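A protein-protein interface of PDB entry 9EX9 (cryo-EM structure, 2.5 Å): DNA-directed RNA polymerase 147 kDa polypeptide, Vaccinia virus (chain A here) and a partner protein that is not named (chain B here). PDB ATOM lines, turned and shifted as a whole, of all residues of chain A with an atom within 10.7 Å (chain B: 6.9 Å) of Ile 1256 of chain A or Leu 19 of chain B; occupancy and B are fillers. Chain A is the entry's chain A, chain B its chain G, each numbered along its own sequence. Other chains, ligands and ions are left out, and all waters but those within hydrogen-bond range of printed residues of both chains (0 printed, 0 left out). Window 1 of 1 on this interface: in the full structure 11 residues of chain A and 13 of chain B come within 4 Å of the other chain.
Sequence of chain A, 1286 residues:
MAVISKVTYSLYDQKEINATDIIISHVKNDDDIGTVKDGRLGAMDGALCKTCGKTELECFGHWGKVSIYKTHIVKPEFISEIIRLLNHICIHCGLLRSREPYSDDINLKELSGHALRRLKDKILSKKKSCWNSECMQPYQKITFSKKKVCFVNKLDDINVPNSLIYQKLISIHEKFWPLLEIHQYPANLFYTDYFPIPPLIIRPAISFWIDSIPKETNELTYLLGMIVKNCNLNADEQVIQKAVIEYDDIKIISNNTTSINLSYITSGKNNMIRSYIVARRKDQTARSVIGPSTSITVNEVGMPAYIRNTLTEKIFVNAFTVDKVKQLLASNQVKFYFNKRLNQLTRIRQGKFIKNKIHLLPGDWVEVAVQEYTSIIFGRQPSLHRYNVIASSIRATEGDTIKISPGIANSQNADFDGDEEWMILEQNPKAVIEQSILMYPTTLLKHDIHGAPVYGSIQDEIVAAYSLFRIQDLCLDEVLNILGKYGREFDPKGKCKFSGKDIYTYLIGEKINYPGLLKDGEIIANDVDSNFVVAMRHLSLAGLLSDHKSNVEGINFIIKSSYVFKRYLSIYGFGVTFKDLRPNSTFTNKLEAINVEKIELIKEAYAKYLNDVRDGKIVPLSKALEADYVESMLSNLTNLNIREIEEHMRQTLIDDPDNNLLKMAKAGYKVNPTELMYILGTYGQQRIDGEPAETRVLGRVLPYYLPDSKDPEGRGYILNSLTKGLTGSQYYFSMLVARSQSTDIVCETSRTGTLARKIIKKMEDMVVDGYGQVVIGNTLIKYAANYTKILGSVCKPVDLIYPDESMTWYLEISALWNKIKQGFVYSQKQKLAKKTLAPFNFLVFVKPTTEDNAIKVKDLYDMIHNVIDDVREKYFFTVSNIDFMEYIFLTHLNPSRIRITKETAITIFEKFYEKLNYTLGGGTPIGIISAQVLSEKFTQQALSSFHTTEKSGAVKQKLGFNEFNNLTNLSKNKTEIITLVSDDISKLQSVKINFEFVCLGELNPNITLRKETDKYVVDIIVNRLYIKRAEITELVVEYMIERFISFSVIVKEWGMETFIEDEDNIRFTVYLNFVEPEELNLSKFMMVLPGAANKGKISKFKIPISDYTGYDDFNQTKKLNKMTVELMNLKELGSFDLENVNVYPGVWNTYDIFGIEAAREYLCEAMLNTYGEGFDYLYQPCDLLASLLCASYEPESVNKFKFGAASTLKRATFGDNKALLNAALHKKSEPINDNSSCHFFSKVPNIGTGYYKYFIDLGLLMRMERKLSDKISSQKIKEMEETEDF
Among the printed residues, pairs that only touch across the chains: Phe 1255 of chain A with Gly 59 of chain B, Tyr 1254 of chain A with Ile 61 of chain B, Asp 1257 of chain A with Leu 58 of chain B, Ile 1256 of chain A with Val 66 of chain B, Ile 1256 of chain A with Leu 19 of chain B, Leu 1258 of chain A with Ile 68 of chain B, Phe 1255 of chain A with Ile 61 of chain B, Phe 1255 of chain A with Glu 60 of chain B, Ile 1256 of chain A with Leu 58 of chain B, Leu 1261 of chain A with Leu 19 of chain B, Arg 1266 of chain A with Leu 21 of chain B and Met 1264 of chain A with Leu 21 of chain B.
Hydrophobic or aromatic side chains of chain A that line the printed part of chain B: Phe 1255, Ile 1256, Leu 1258, Leu 1261 and Met 1264.
Of the 19 printed residues of chain B, 10 touch a printed residue of chain A.
Hydrophobic or aromatic side chains of chain B within 4 Å of the printed part of chain A: His 17, Leu 19, Leu 21, Leu 58, Ile 61, Val 66 and Ile 68.
Among the printed residues, 15 pairs touch across the chains.
Of the printed residues of chain A, Leu 19 of chain B touches Ile 1256 (3.7 Å) and Leu 1261 (3.9 Å).
No residue of chain A comes within 4 Å of Pro 16 of chain B.
Of the printed residues of chain A, Leu 58 of chain B touches Ile 1256 (3.9 Å) and Asp 1257 (3.7 Å).
Gly 59 of chain B touches two residues of chain A.
Of the printed residues of chain B, Asp 1257 of chain A touches Leu 58.
Of the printed residues of chain B, Arg 1266 of chain A touches Leu 21 and Asp 22.
Of the printed residues of chain A, Leu 21 of chain B touches Met 1264 and Arg 1266.
Of the printed residues of chain B, Leu 1258 of chain A touches Ile 68.
Glu 15 of chain B touches none of the printed residues of chain A.
The nearest residue of chain B that does not touch Ile 1256 of chain A is Ile 61 of chain B (4.2 Å).
The nearest residue of chain A that does not touch Leu 19 of chain B is Leu 1258 of chain A (4.2 Å).
NH1 of Arg 341 of chain A lies within hydrogen-bond range of NE2 of His 17 of chain B.
O of Gly 59 of chain B lies within hydrogen-bond range of N of Ile 1256 of chain A (2.8 Å).
The guanidinium group of Arg 1266 of chain A is in salt-bridge range of the side-chain carboxylate of Asp 22 of chain B (2.6 Å).
N of Gly 1259 of chain A sits at hydrogen-bond distance from OD1 of Asp 1257 of chain A (3.2 Å).
N of Leu 14 of chain B is in hydrogen-bond range of O of Val 66 of chain B (2.9 Å).
O of Asp 22 of chain B lies close to OD1 of Asn 26 of chain B, 2.5 Å away.
N of Val 67 of chain B lies within hydrogen-bond range of O of Glu 60 of chain B (2.9 Å).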
ATOM      1  N   ARG A 341     -14.976  10.726   7.179  1.00  0.00           N
ATOM      2  CA  ARG A 341     -16.291  10.321   7.652  1.00  0.00           C
ATOM      3  C   ARG A 341     -17.241  11.500   7.779  1.00  0.00           C
ATOM      4  O   ARG A 341     -18.453  11.292   7.892  1.00  0.00           O
ATOM      5  CB  ARG A 341     -16.158   9.595   8.988  1.00  0.00           C
ATOM      6  CG  ARG A 341     -15.278   8.363   8.912  1.00  0.00           C
ATOM      7  CD  ARG A 341     -15.034   7.767  10.281  1.00  0.00           C
ATOM      8  NE  ARG A 341     -13.973   6.767  10.254  1.00  0.00           N
ATOM      9  CZ  ARG A 341     -14.154   5.481   9.987  1.00  0.00           C
ATOM     10  NH1 ARG A 341     -15.354   4.993   9.718  1.00  0.00           N
ATOM     11  NH2 ARG A 341     -13.105   4.665   9.986  1.00  0.00           N
ATOM     12  N   PRO A 362      -8.613   5.483   9.998  1.00  0.00           N
ATOM     13  CA  PRO A 362      -8.222   5.006   8.667  1.00  0.00           C
ATOM     14  C   PRO A 362      -9.115   5.583   7.581  1.00  0.00           C
ATOM     15  O   PRO A 362     -10.326   5.728   7.758  1.00  0.00           O
ATOM     16  CB  PRO A 362      -8.378   3.485   8.772  1.00  0.00           C
ATOM     17  CG  PRO A 362      -8.263   3.193  10.213  1.00  0.00           C
ATOM     18  CD  PRO A 362      -8.852   4.367  10.927  1.00  0.00           C
ATOM     19  N   GLY A 363      -8.504   5.903   6.443  1.00  0.00           N
ATOM     20  CA  GLY A 363      -9.186   6.524   5.333  1.00  0.00           C
ATOM     21  C   GLY A 363      -9.052   8.030   5.277  1.00  0.00           C
ATOM     22  O   GLY A 363      -9.304   8.621   4.224  1.00  0.00           O
ATOM     23  N   LYS A 430      -4.298   5.532  -7.605  1.00  0.00           N
ATOM     24  CA  LYS A 430      -4.293   4.936  -8.935  1.00  0.00           C
ATOM     25  C   LYS A 430      -3.535   5.814  -9.917  1.00  0.00           C
ATOM     26  O   LYS A 430      -2.726   5.322 -10.717  1.00  0.00           O
ATOM     27  CB  LYS A 430      -5.722   4.721  -9.421  1.00  0.00           C
ATOM     28  CG  LYS A 430      -6.527   3.784  -8.562  1.00  0.00           C
ATOM     29  CD  LYS A 430      -7.912   3.590  -9.123  1.00  0.00           C
ATOM     30  CE  LYS A 430      -8.756   2.736  -8.211  1.00  0.00           C
ATOM     31  NZ  LYS A 430     -10.167   2.663  -8.661  1.00  0.00           N
ATOM     32  N   LYS A1253     -12.507  -4.471 -16.711  1.00  0.00           N
ATOM     33  CA  LYS A1253     -13.369  -4.297 -15.552  1.00  0.00           C
ATOM     34  C   LYS A1253     -12.807  -5.098 -14.387  1.00  0.00           C
ATOM     35  O   LYS A1253     -12.417  -6.257 -14.554  1.00  0.00           O
ATOM     36  CB  LYS A1253     -14.797  -4.739 -15.867  1.00  0.00           C
ATOM     37  CG  LYS A1253     -15.812  -4.361 -14.808  1.00  0.00           C
ATOM     38  CD  LYS A1253     -17.224  -4.709 -15.249  1.00  0.00           C
ATOM     39  CE  LYS A1253     -18.220  -4.579 -14.107  1.00  0.00           C
ATOM     40  NZ  LYS A1253     -18.287  -3.199 -13.558  1.00  0.00           N
ATOM     41  N   TYR A1254     -12.771  -4.482 -13.209  1.00  0.00           N
ATOM     42  CA  TYR A1254     -12.092  -5.036 -12.046  1.00  0.00           C
ATOM     43  C   TYR A1254     -13.084  -5.380 -10.942  1.00  0.00           C
ATOM     44  O   TYR A1254     -14.037  -4.637 -10.694  1.00  0.00           O
ATOM     45  CB  TYR A1254     -11.053  -4.049 -11.518  1.00  0.00           C
ATOM     46  CG  TYR A1254     -10.037  -3.653 -12.559  1.00  0.00           C
ATOM     47  CD1 TYR A1254      -8.916  -4.431 -12.791  1.00  0.00           C
ATOM     48  CD2 TYR A1254     -10.205  -2.509 -13.321  1.00  0.00           C
ATOM     49  CE1 TYR A1254      -7.990  -4.078 -13.747  1.00  0.00           C
ATOM     50  CE2 TYR A1254      -9.283  -2.150 -14.277  1.00  0.00           C
ATOM     51  CZ  TYR A1254      -8.178  -2.937 -14.485  1.00  0.00           C
ATOM     52  OH  TYR A1254      -7.257  -2.585 -15.436  1.00  0.00           O
ATOM     53  N   PHE A1255     -12.849  -6.513 -10.284  1.00  0.00           N
ATOM     54  CA  PHE A1255     -13.620  -6.958  -9.134  1.00  0.00           C
ATOM     55  C   PHE A1255     -12.665  -7.214  -7.977  1.00  0.00           C
ATOM     56  O   PHE A1255     -11.447  -7.106  -8.118  1.00  0.00           O
ATOM     57  CB  PHE A1255     -14.414  -8.232  -9.443  1.00  0.00           C
ATOM     58  CG  PHE A1255     -15.299  -8.120 -10.644  1.00  0.00           C
ATOM     59  CD1 PHE A1255     -14.784  -8.272 -11.912  1.00  0.00           C
ATOM     60  CD2 PHE A1255     -16.648  -7.878 -10.503  1.00  0.00           C
ATOM     61  CE1 PHE A1255     -15.596  -8.176 -13.015  1.00  0.00           C
ATOM     62  CE2 PHE A1255     -17.461  -7.781 -11.605  1.00  0.00           C
ATOM     63  CZ  PHE A1255     -16.934  -7.929 -12.860  1.00  0.00           C
ATOM     64  N   ILE A1256     -13.222  -7.559  -6.822  1.00  0.00           N
ATOM     65  CA  ILE A1256     -12.432  -7.943  -5.658  1.00  0.00           C
ATOM     66  C   ILE A1256     -12.981  -9.259  -5.125  1.00  0.00           C
ATOM     67  O   ILE A1256     -14.192  -9.397  -4.929  1.00  0.00           O
ATOM     68  CB  ILE A1256     -12.445  -6.860  -4.564  1.00  0.00           C
ATOM     69  CG1 ILE A1256     -11.630  -7.320  -3.357  1.00  0.00           C
ATOM     70  CG2 ILE A1256     -13.862  -6.541  -4.140  1.00  0.00           C
ATOM     71  CD1 ILE A1256     -11.419  -6.248  -2.326  1.00  0.00           C
ATOM     72  N   ASP A1257     -12.090 -10.218  -4.888  1.00  0.00           N
ATOM     73  CA  ASP A1257     -12.465 -11.560  -4.461  1.00  0.00           C
ATOM     74  C   ASP A1257     -12.356 -11.639  -2.944  1.00  0.00           C
ATOM     75  O   ASP A1257     -11.250 -11.646  -2.395  1.00  0.00           O
ATOM     76  CB  ASP A1257     -11.575 -12.603  -5.128  1.00  0.00           C
ATOM     77  CG  ASP A1257     -12.051 -14.013  -4.882  1.00  0.00           C
ATOM     78  OD1 ASP A1257     -13.098 -14.176  -4.227  1.00  0.00           O
ATOM     79  OD2 ASP A1257     -11.379 -14.958  -5.344  1.00  0.00           O
ATOM     80  N   LEU A1258     -13.499 -11.715  -2.274  1.00  0.00           N
ATOM     81  CA  LEU A1258     -13.554 -11.728  -0.819  1.00  0.00           C
ATOM     82  C   LEU A1258     -13.478 -13.130  -0.233  1.00  0.00           C
ATOM     83  O   LEU A1258     -13.574 -13.278   0.988  1.00  0.00           O
ATOM     84  CB  LEU A1258     -14.841 -11.048  -0.344  1.00  0.00           C
ATOM     85  CG  LEU A1258     -15.041  -9.601  -0.797  1.00  0.00           C
ATOM     86  CD1 LEU A1258     -16.409  -9.099  -0.395  1.00  0.00           C
ATOM     87  CD2 LEU A1258     -13.961  -8.713  -0.215  1.00  0.00           C
ATOM     88  N   GLY A1259     -13.303 -14.158  -1.063  1.00  0.00           N
ATOM     89  CA  GLY A1259     -13.332 -15.518  -0.551  1.00  0.00           C
ATOM     90  C   GLY A1259     -12.273 -15.772   0.503  1.00  0.00           C
ATOM     91  O   GLY A1259     -12.558 -16.332   1.564  1.00  0.00           O
ATOM     92  N   LEU A1260     -11.034 -15.364   0.229  1.00  0.00           N
ATOM     93  CA  LEU A1260      -9.954 -15.631   1.175  1.00  0.00           C
ATOM     94  C   LEU A1260     -10.143 -14.850   2.468  1.00  0.00           C
ATOM     95  O   LEU A1260      -9.892 -15.375   3.558  1.00  0.00           O
ATOM     96  CB  LEU A1260      -8.605 -15.296   0.545  1.00  0.00           C
ATOM     97  CG  LEU A1260      -7.393 -15.523   1.454  1.00  0.00           C
ATOM     98  CD1 LEU A1260      -7.367 -16.949   1.969  1.00  0.00           C
ATOM     99  CD2 LEU A1260      -6.106 -15.205   0.721  1.00  0.00           C
ATOM    100  N   LEU A1261     -10.572 -13.591   2.371  1.00  0.00           N
ATOM    101  CA  LEU A1261     -10.721 -12.770   3.567  1.00  0.00           C
ATOM    102  C   LEU A1261     -11.761 -13.354   4.509  1.00  0.00           C
ATOM    103  O   LEU A1261     -11.575 -13.352   5.730  1.00  0.00           O
ATOM    104  CB  LEU A1261     -11.097 -11.341   3.176  1.00  0.00           C
ATOM    105  CG  LEU A1261     -11.341 -10.369   4.329  1.00  0.00           C
ATOM    106  CD1 LEU A1261     -10.064 -10.114   5.102  1.00  0.00           C
ATOM    107  CD2 LEU A1261     -11.917  -9.075   3.802  1.00  0.00           C
ATOM    108  N   MET A1262     -12.870 -13.851   3.964  1.00  0.00           N
ATOM    109  CA  MET A1262     -13.925 -14.415   4.793  1.00  0.00           C
ATOM    110  C   MET A1262     -13.577 -15.793   5.338  1.00  0.00           C
ATOM    111  O   MET A1262     -14.313 -16.306   6.186  1.00  0.00           O
ATOM    112  CB  MET A1262     -15.230 -14.487   4.000  1.00  0.00           C
ATOM    113  CG  MET A1262     -15.744 -13.126   3.568  1.00  0.00           C
ATOM    114  SD  MET A1262     -17.392 -13.175   2.851  1.00  0.00           S
ATOM    115  CE  MET A1262     -18.376 -13.567   4.291  1.00  0.00           C
ATOM    116  N   MET A1264     -10.728 -16.278   6.956  1.00  0.00           N
ATOM    117  CA  MET A1264      -9.867 -16.011   8.097  1.00  0.00           C
ATOM    118  C   MET A1264     -10.728 -15.702   9.314  1.00  0.00           C
ATOM    119  O   MET A1264     -11.790 -15.086   9.193  1.00  0.00           O
ATOM    120  CB  MET A1264      -8.927 -14.839   7.815  1.00  0.00           C
ATOM    121  CG  MET A1264      -7.973 -15.067   6.661  1.00  0.00           C
ATOM    122  SD  MET A1264      -6.863 -13.670   6.395  1.00  0.00           S
ATOM    123  CE  MET A1264      -5.903 -14.260   5.004  1.00  0.00           C
ATOM    124  N   ARG A1266     -10.599 -14.459  13.565  1.00  0.00           N
ATOM    125  CA  ARG A1266      -9.809 -13.795  14.594  1.00  0.00           C
ATOM    126  C   ARG A1266      -9.467 -14.756  15.725  1.00  0.00           C
ATOM    127  O   ARG A1266      -8.352 -14.741  16.247  1.00  0.00           O
ATOM    128  CB  ARG A1266     -10.561 -12.582  15.145  1.00  0.00           C
ATOM    129  CG  ARG A1266      -9.772 -11.775  16.163  1.00  0.00           C
ATOM    130  CD  ARG A1266     -10.491 -10.486  16.528  1.00  0.00           C
ATOM    131  NE  ARG A1266     -10.555  -9.556  15.409  1.00  0.00           N
ATOM    132  CZ  ARG A1266     -11.153  -8.372  15.449  1.00  0.00           C
ATOM    133  NH1 ARG A1266     -11.758  -7.939  16.543  1.00  0.00           N
ATOM    134  NH2 ARG A1266     -11.144  -7.603  14.364  1.00  0.00           N
ATOM    135  N   LEU B  14     -19.586  -0.865   0.573  1.00  0.00           N
ATOM    136  CA  LEU B  14     -18.619  -0.891   1.658  1.00  0.00           C
ATOM    137  C   LEU B  14     -17.413  -0.032   1.307  1.00  0.00           C
ATOM    138  O   LEU B  14     -17.074   0.145   0.131  1.00  0.00           O
ATOM    139  CB  LEU B  14     -18.141  -2.315   1.960  1.00  0.00           C
ATOM    140  CG  LEU B  14     -19.123  -3.280   2.622  1.00  0.00           C
ATOM    141  CD1 LEU B  14     -20.203  -3.717   1.654  1.00  0.00           C
ATOM    142  CD2 LEU B  14     -18.377  -4.479   3.163  1.00  0.00           C
ATOM    143  N   GLU B  15     -16.770   0.497   2.341  1.00  0.00           N
ATOM    144  CA  GLU B  15     -15.550   1.274   2.219  1.00  0.00           C
ATOM    145  C   GLU B  15     -14.334   0.382   2.416  1.00  0.00           C
ATOM    146  O   GLU B  15     -14.420  -0.669   3.052  1.00  0.00           O
ATOM    147  CB  GLU B  15     -15.532   2.401   3.253  1.00  0.00           C
ATOM    148  CG  GLU B  15     -16.739   3.315   3.180  1.00  0.00           C
ATOM    149  CD  GLU B  15     -16.874   3.998   1.835  1.00  0.00           C
ATOM    150  OE1 GLU B  15     -15.848   4.167   1.147  1.00  0.00           O
ATOM    151  OE2 GLU B  15     -18.008   4.363   1.463  1.00  0.00           O
ATOM    152  N   PRO B  16     -13.177   0.764   1.873  1.00  0.00           N
ATOM    153  CA  PRO B  16     -11.996  -0.099   2.028  1.00  0.00           C
ATOM    154  C   PRO B  16     -11.631  -0.383   3.474  1.00  0.00           C
ATOM    155  O   PRO B  16     -11.210  -1.502   3.786  1.00  0.00           O
ATOM    156  CB  PRO B  16     -10.896   0.688   1.306  1.00  0.00           C
ATOM    157  CG  PRO B  16     -11.616   1.524   0.332  1.00  0.00           C
ATOM    158  CD  PRO B  16     -12.900   1.909   0.994  1.00  0.00           C
ATOM    159  N   HIS B  17     -11.788   0.589   4.376  1.00  0.00           N
ATOM    160  CA  HIS B  17     -11.379   0.368   5.757  1.00  0.00           C
ATOM    161  C   HIS B  17     -12.241  -0.670   6.460  1.00  0.00           C
ATOM    162  O   HIS B  17     -11.884  -1.099   7.560  1.00  0.00           O
ATOM    163  CB  HIS B  17     -11.401   1.682   6.540  1.00  0.00           C
ATOM    164  CG  HIS B  17     -12.775   2.181   6.856  1.00  0.00           C
ATOM    165  ND1 HIS B  17     -13.462   3.042   6.029  1.00  0.00           N
ATOM    166  CD2 HIS B  17     -13.585   1.953   7.917  1.00  0.00           C
ATOM    167  CE1 HIS B  17     -14.640   3.315   6.562  1.00  0.00           C
ATOM    168  NE2 HIS B  17     -14.738   2.667   7.708  1.00  0.00           N
ATOM    169  N   GLU B  18     -13.355  -1.075   5.858  1.00  0.00           N
ATOM    170  CA  GLU B  18     -14.207  -2.120   6.404  1.00  0.00           C
ATOM    171  C   GLU B  18     -13.865  -3.503   5.872  1.00  0.00           C
ATOM    172  O   GLU B  18     -14.538  -4.471   6.235  1.00  0.00           O
ATOM    173  CB  GLU B  18     -15.674  -1.810   6.100  1.00  0.00           C
ATOM    174  CG  GLU B  18     -16.194  -0.578   6.809  1.00  0.00           C
ATOM    175  CD  GLU B  18     -17.603  -0.225   6.397  1.00  0.00           C
ATOM    176  OE1 GLU B  18     -18.030  -0.661   5.311  1.00  0.00           O
ATOM    177  OE2 GLU B  18     -18.286   0.490   7.157  1.00  0.00           O
ATOM    178  N   LEU B  19     -12.845  -3.623   5.023  1.00  0.00           N
ATOM    179  CA  LEU B  19     -12.423  -4.920   4.496  1.00  0.00           C
ATOM    180  C   LEU B  19     -11.370  -5.546   5.410  1.00  0.00           C
ATOM    181  O   LEU B  19     -10.231  -5.795   5.027  1.00  0.00           O
ATOM    182  CB  LEU B  19     -11.895  -4.769   3.075  1.00  0.00           C
ATOM    183  CG  LEU B  19     -12.865  -4.254   2.014  1.00  0.00           C
ATOM    184  CD1 LEU B  19     -12.171  -4.181   0.669  1.00  0.00           C
ATOM    185  CD2 LEU B  19     -14.099  -5.128   1.924  1.00  0.00           C
ATOM    186  N   THR B  20     -11.786  -5.805   6.647  1.00  0.00           N
ATOM    187  CA  THR B  20     -10.912  -6.401   7.649  1.00  0.00           C
ATOM    188  C   THR B  20     -11.568  -7.650   8.221  1.00  0.00           C
ATOM    189  O   THR B  20     -12.542  -8.155   7.656  1.00  0.00           O
ATOM    190  CB  THR B  20     -10.599  -5.402   8.763  1.00  0.00           C
ATOM    191  OG1 THR B  20     -11.804  -5.063   9.459  1.00  0.00           O
ATOM    192  CG2 THR B  20      -9.985  -4.140   8.194  1.00  0.00           C
ATOM    193  N   LEU B  21     -11.034  -8.168   9.327  1.00  0.00           N
ATOM    194  CA  LEU B  21     -11.602  -9.371   9.925  1.00  0.00           C
ATOM    195  C   LEU B  21     -13.059  -9.186  10.329  1.00  0.00           C
ATOM    196  O   LEU B  21     -13.780 -10.179  10.469  1.00  0.00           O
ATOM    197  CB  LEU B  21     -10.780  -9.792  11.142  1.00  0.00           C
ATOM    198  CG  LEU B  21      -9.369 -10.295  10.847  1.00  0.00           C
ATOM    199  CD1 LEU B  21      -8.635 -10.604  12.135  1.00  0.00           C
ATOM    200  CD2 LEU B  21      -9.414 -11.521   9.956  1.00  0.00           C
ATOM    201  N   ASP B  22     -13.508  -7.950  10.522  1.00  0.00           N
ATOM    202  CA  ASP B  22     -14.908  -7.681  10.846  1.00  0.00           C
ATOM    203  C   ASP B  22     -15.734  -7.478   9.582  1.00  0.00           C
ATOM    204  O   ASP B  22     -16.502  -6.529   9.466  1.00  0.00           O
ATOM    205  CB  ASP B  22     -15.003  -6.462  11.754  1.00  0.00           C
ATOM    206  CG  ASP B  22     -14.033  -6.523  12.908  1.00  0.00           C
ATOM    207  OD1 ASP B  22     -13.497  -7.615  13.177  1.00  0.00           O
ATOM    208  OD2 ASP B  22     -13.808  -5.478  13.552  1.00  0.00           O
ATOM    209  N   ILE B  23     -15.593  -8.391   8.626  1.00  0.00           N
ATOM    210  CA  ILE B  23     -16.261  -8.225   7.341  1.00  0.00           C
ATOM    211  C   ILE B  23     -17.729  -8.625   7.440  1.00  0.00           C
ATOM    212  O   ILE B  23     -18.616  -7.907   6.965  1.00  0.00           O
ATOM    213  CB  ILE B  23     -15.514  -9.018   6.247  1.00  0.00           C
ATOM    214  CG1 ILE B  23     -16.206  -8.871   4.890  1.00  0.00           C
ATOM    215  CG2 ILE B  23     -15.398 -10.493   6.605  1.00  0.00           C
ATOM    216  CD1 ILE B  23     -16.250  -7.461   4.375  1.00  0.00           C
ATOM    217  N   ASN B  26     -19.763  -6.001   9.369  1.00  0.00           N
ATOM    218  CA  ASN B  26     -20.039  -4.808   8.580  1.00  0.00           C
ATOM    219  C   ASN B  26     -21.094  -5.086   7.522  1.00  0.00           C
ATOM    220  O   ASN B  26     -21.972  -4.249   7.281  1.00  0.00           O
ATOM    221  CB  ASN B  26     -18.754  -4.291   7.940  1.00  0.00           C
ATOM    222  CG  ASN B  26     -17.713  -3.880   8.963  1.00  0.00           C
ATOM    223  OD1 ASN B  26     -16.521  -4.115   8.776  1.00  0.00           O
ATOM    224  ND2 ASN B  26     -18.157  -3.263  10.052  1.00  0.00           N
ATOM    225  N   PRO B  57     -20.923 -13.737  -4.195  1.00  0.00           N
ATOM    226  CA  PRO B  57     -20.434 -13.271  -5.498  1.00  0.00           C
ATOM    227  C   PRO B  57     -19.286 -12.285  -5.342  1.00  0.00           C
ATOM    228  O   PRO B  57     -19.026 -11.745  -4.267  1.00  0.00           O
ATOM    229  CB  PRO B  57     -21.658 -12.600  -6.127  1.00  0.00           C
ATOM    230  CG  PRO B  57     -22.820 -13.096  -5.358  1.00  0.00           C
ATOM    231  CD  PRO B  57     -22.330 -13.361  -3.980  1.00  0.00           C
ATOM    232  N   LEU B  58     -18.590 -12.049  -6.452  1.00  0.00           N
ATOM    233  CA  LEU B  58     -17.502 -11.081  -6.453  1.00  0.00           C
ATOM    234  C   LEU B  58     -18.037  -9.678  -6.197  1.00  0.00           C
ATOM    235  O   LEU B  58     -19.183  -9.358  -6.519  1.00  0.00           O
ATOM    236  CB  LEU B  58     -16.756 -11.107  -7.787  1.00  0.00           C
ATOM    237  CG  LEU B  58     -15.923 -12.340  -8.124  1.00  0.00           C
ATOM    238  CD1 LEU B  58     -15.378 -12.217  -9.527  1.00  0.00           C
ATOM    239  CD2 LEU B  58     -14.795 -12.517  -7.134  1.00  0.00           C
ATOM    240  N   GLY B  59     -17.189  -8.835  -5.614  1.00  0.00           N
ATOM    241  CA  GLY B  59     -17.534  -7.442  -5.394  1.00  0.00           C
ATOM    242  C   GLY B  59     -17.004  -6.556  -6.511  1.00  0.00           C
ATOM    243  O   GLY B  59     -15.928  -6.790  -7.050  1.00  0.00           O
ATOM    244  N   GLU B  60     -17.780  -5.529  -6.845  1.00  0.00           N
ATOM    245  CA  GLU B  60     -17.439  -4.606  -7.920  1.00  0.00           C
ATOM    246  C   GLU B  60     -16.782  -3.363  -7.341  1.00  0.00           C
ATOM    247  O   GLU B  60     -17.325  -2.742  -6.427  1.00  0.00           O
ATOM    248  CB  GLU B  60     -18.683  -4.210  -8.710  1.00  0.00           C
ATOM    249  CG  GLU B  60     -19.420  -5.373  -9.318  1.00  0.00           C
ATOM    250  CD  GLU B  60     -20.605  -4.929 -10.144  1.00  0.00           C
ATOM    251  OE1 GLU B  60     -20.779  -3.705 -10.321  1.00  0.00           O
ATOM    252  OE2 GLU B  60     -21.362  -5.804 -10.616  1.00  0.00           O
ATOM    253  N   ILE B  61     -15.628  -2.997  -7.880  1.00  0.00           N
ATOM    254  CA  ILE B  61     -14.905  -1.818  -7.422  1.00  0.00           C
ATOM    255  C   ILE B  61     -15.395  -0.623  -8.224  1.00  0.00           C
ATOM    256  O   ILE B  61     -15.297  -0.610  -9.454  1.00  0.00           O
ATOM    257  CB  ILE B  61     -13.389  -2.003  -7.570  1.00  0.00           C
ATOM    258  CG1 ILE B  61     -12.939  -3.249  -6.810  1.00  0.00           C
ATOM    259  CG2 ILE B  61     -12.660  -0.774  -7.054  1.00  0.00           C
ATOM    260  CD1 ILE B  61     -11.471  -3.533  -6.913  1.00  0.00           C
ATOM    261  N   VAL B  66     -16.649  -0.467  -2.717  1.00  0.00           N
ATOM    262  CA  VAL B  66     -16.933  -1.822  -3.171  1.00  0.00           C
ATOM    263  C   VAL B  66     -18.433  -2.055  -3.090  1.00  0.00           C
ATOM    264  O   VAL B  66     -19.092  -1.596  -2.155  1.00  0.00           O
ATOM    265  CB  VAL B  66     -16.170  -2.867  -2.335  1.00  0.00           C
ATOM    266  CG1 VAL B  66     -16.457  -4.266  -2.841  1.00  0.00           C
ATOM    267  CG2 VAL B  66     -14.687  -2.579  -2.373  1.00  0.00           C
ATOM    268  N   VAL B  67     -18.969  -2.761  -4.081  1.00  0.00           N
ATOM    269  CA  VAL B  67     -20.387  -3.076  -4.169  1.00  0.00           C
ATOM    270  C   VAL B  67     -20.541  -4.586  -4.080  1.00  0.00           C
ATOM    271  O   VAL B  67     -19.883  -5.325  -4.821  1.00  0.00           O
ATOM    272  CB  VAL B  67     -21.003  -2.540  -5.473  1.00  0.00           C
ATOM    273  CG1 VAL B  67     -22.396  -3.100  -5.675  1.00  0.00           C
ATOM    274  CG2 VAL B  67     -21.036  -1.028  -5.450  1.00  0.00           C
ATOM    275  N   ILE B  68     -21.410  -5.040  -3.181  1.00  0.00           N
ATOM    276  CA  ILE B  68     -21.579  -6.457  -2.890  1.00  0.00           C
ATOM    277  C   ILE B  68     -23.054  -6.813  -2.979  1.00  0.00           C
ATOM    278  O   ILE B  68     -23.915  -6.056  -2.518  1.00  0.00           O
ATOM    279  CB  ILE B  68     -21.031  -6.818  -1.496  1.00  0.00           C
ATOM    280  CG1 ILE B  68     -19.647  -6.211  -1.290  1.00  0.00           C
ATOM    281  CG2 ILE B  68     -20.965  -8.322  -1.333  1.00  0.00           C
ATOM    282  CD1 ILE B  68     -19.061  -6.494   0.069  1.00  0.00           C
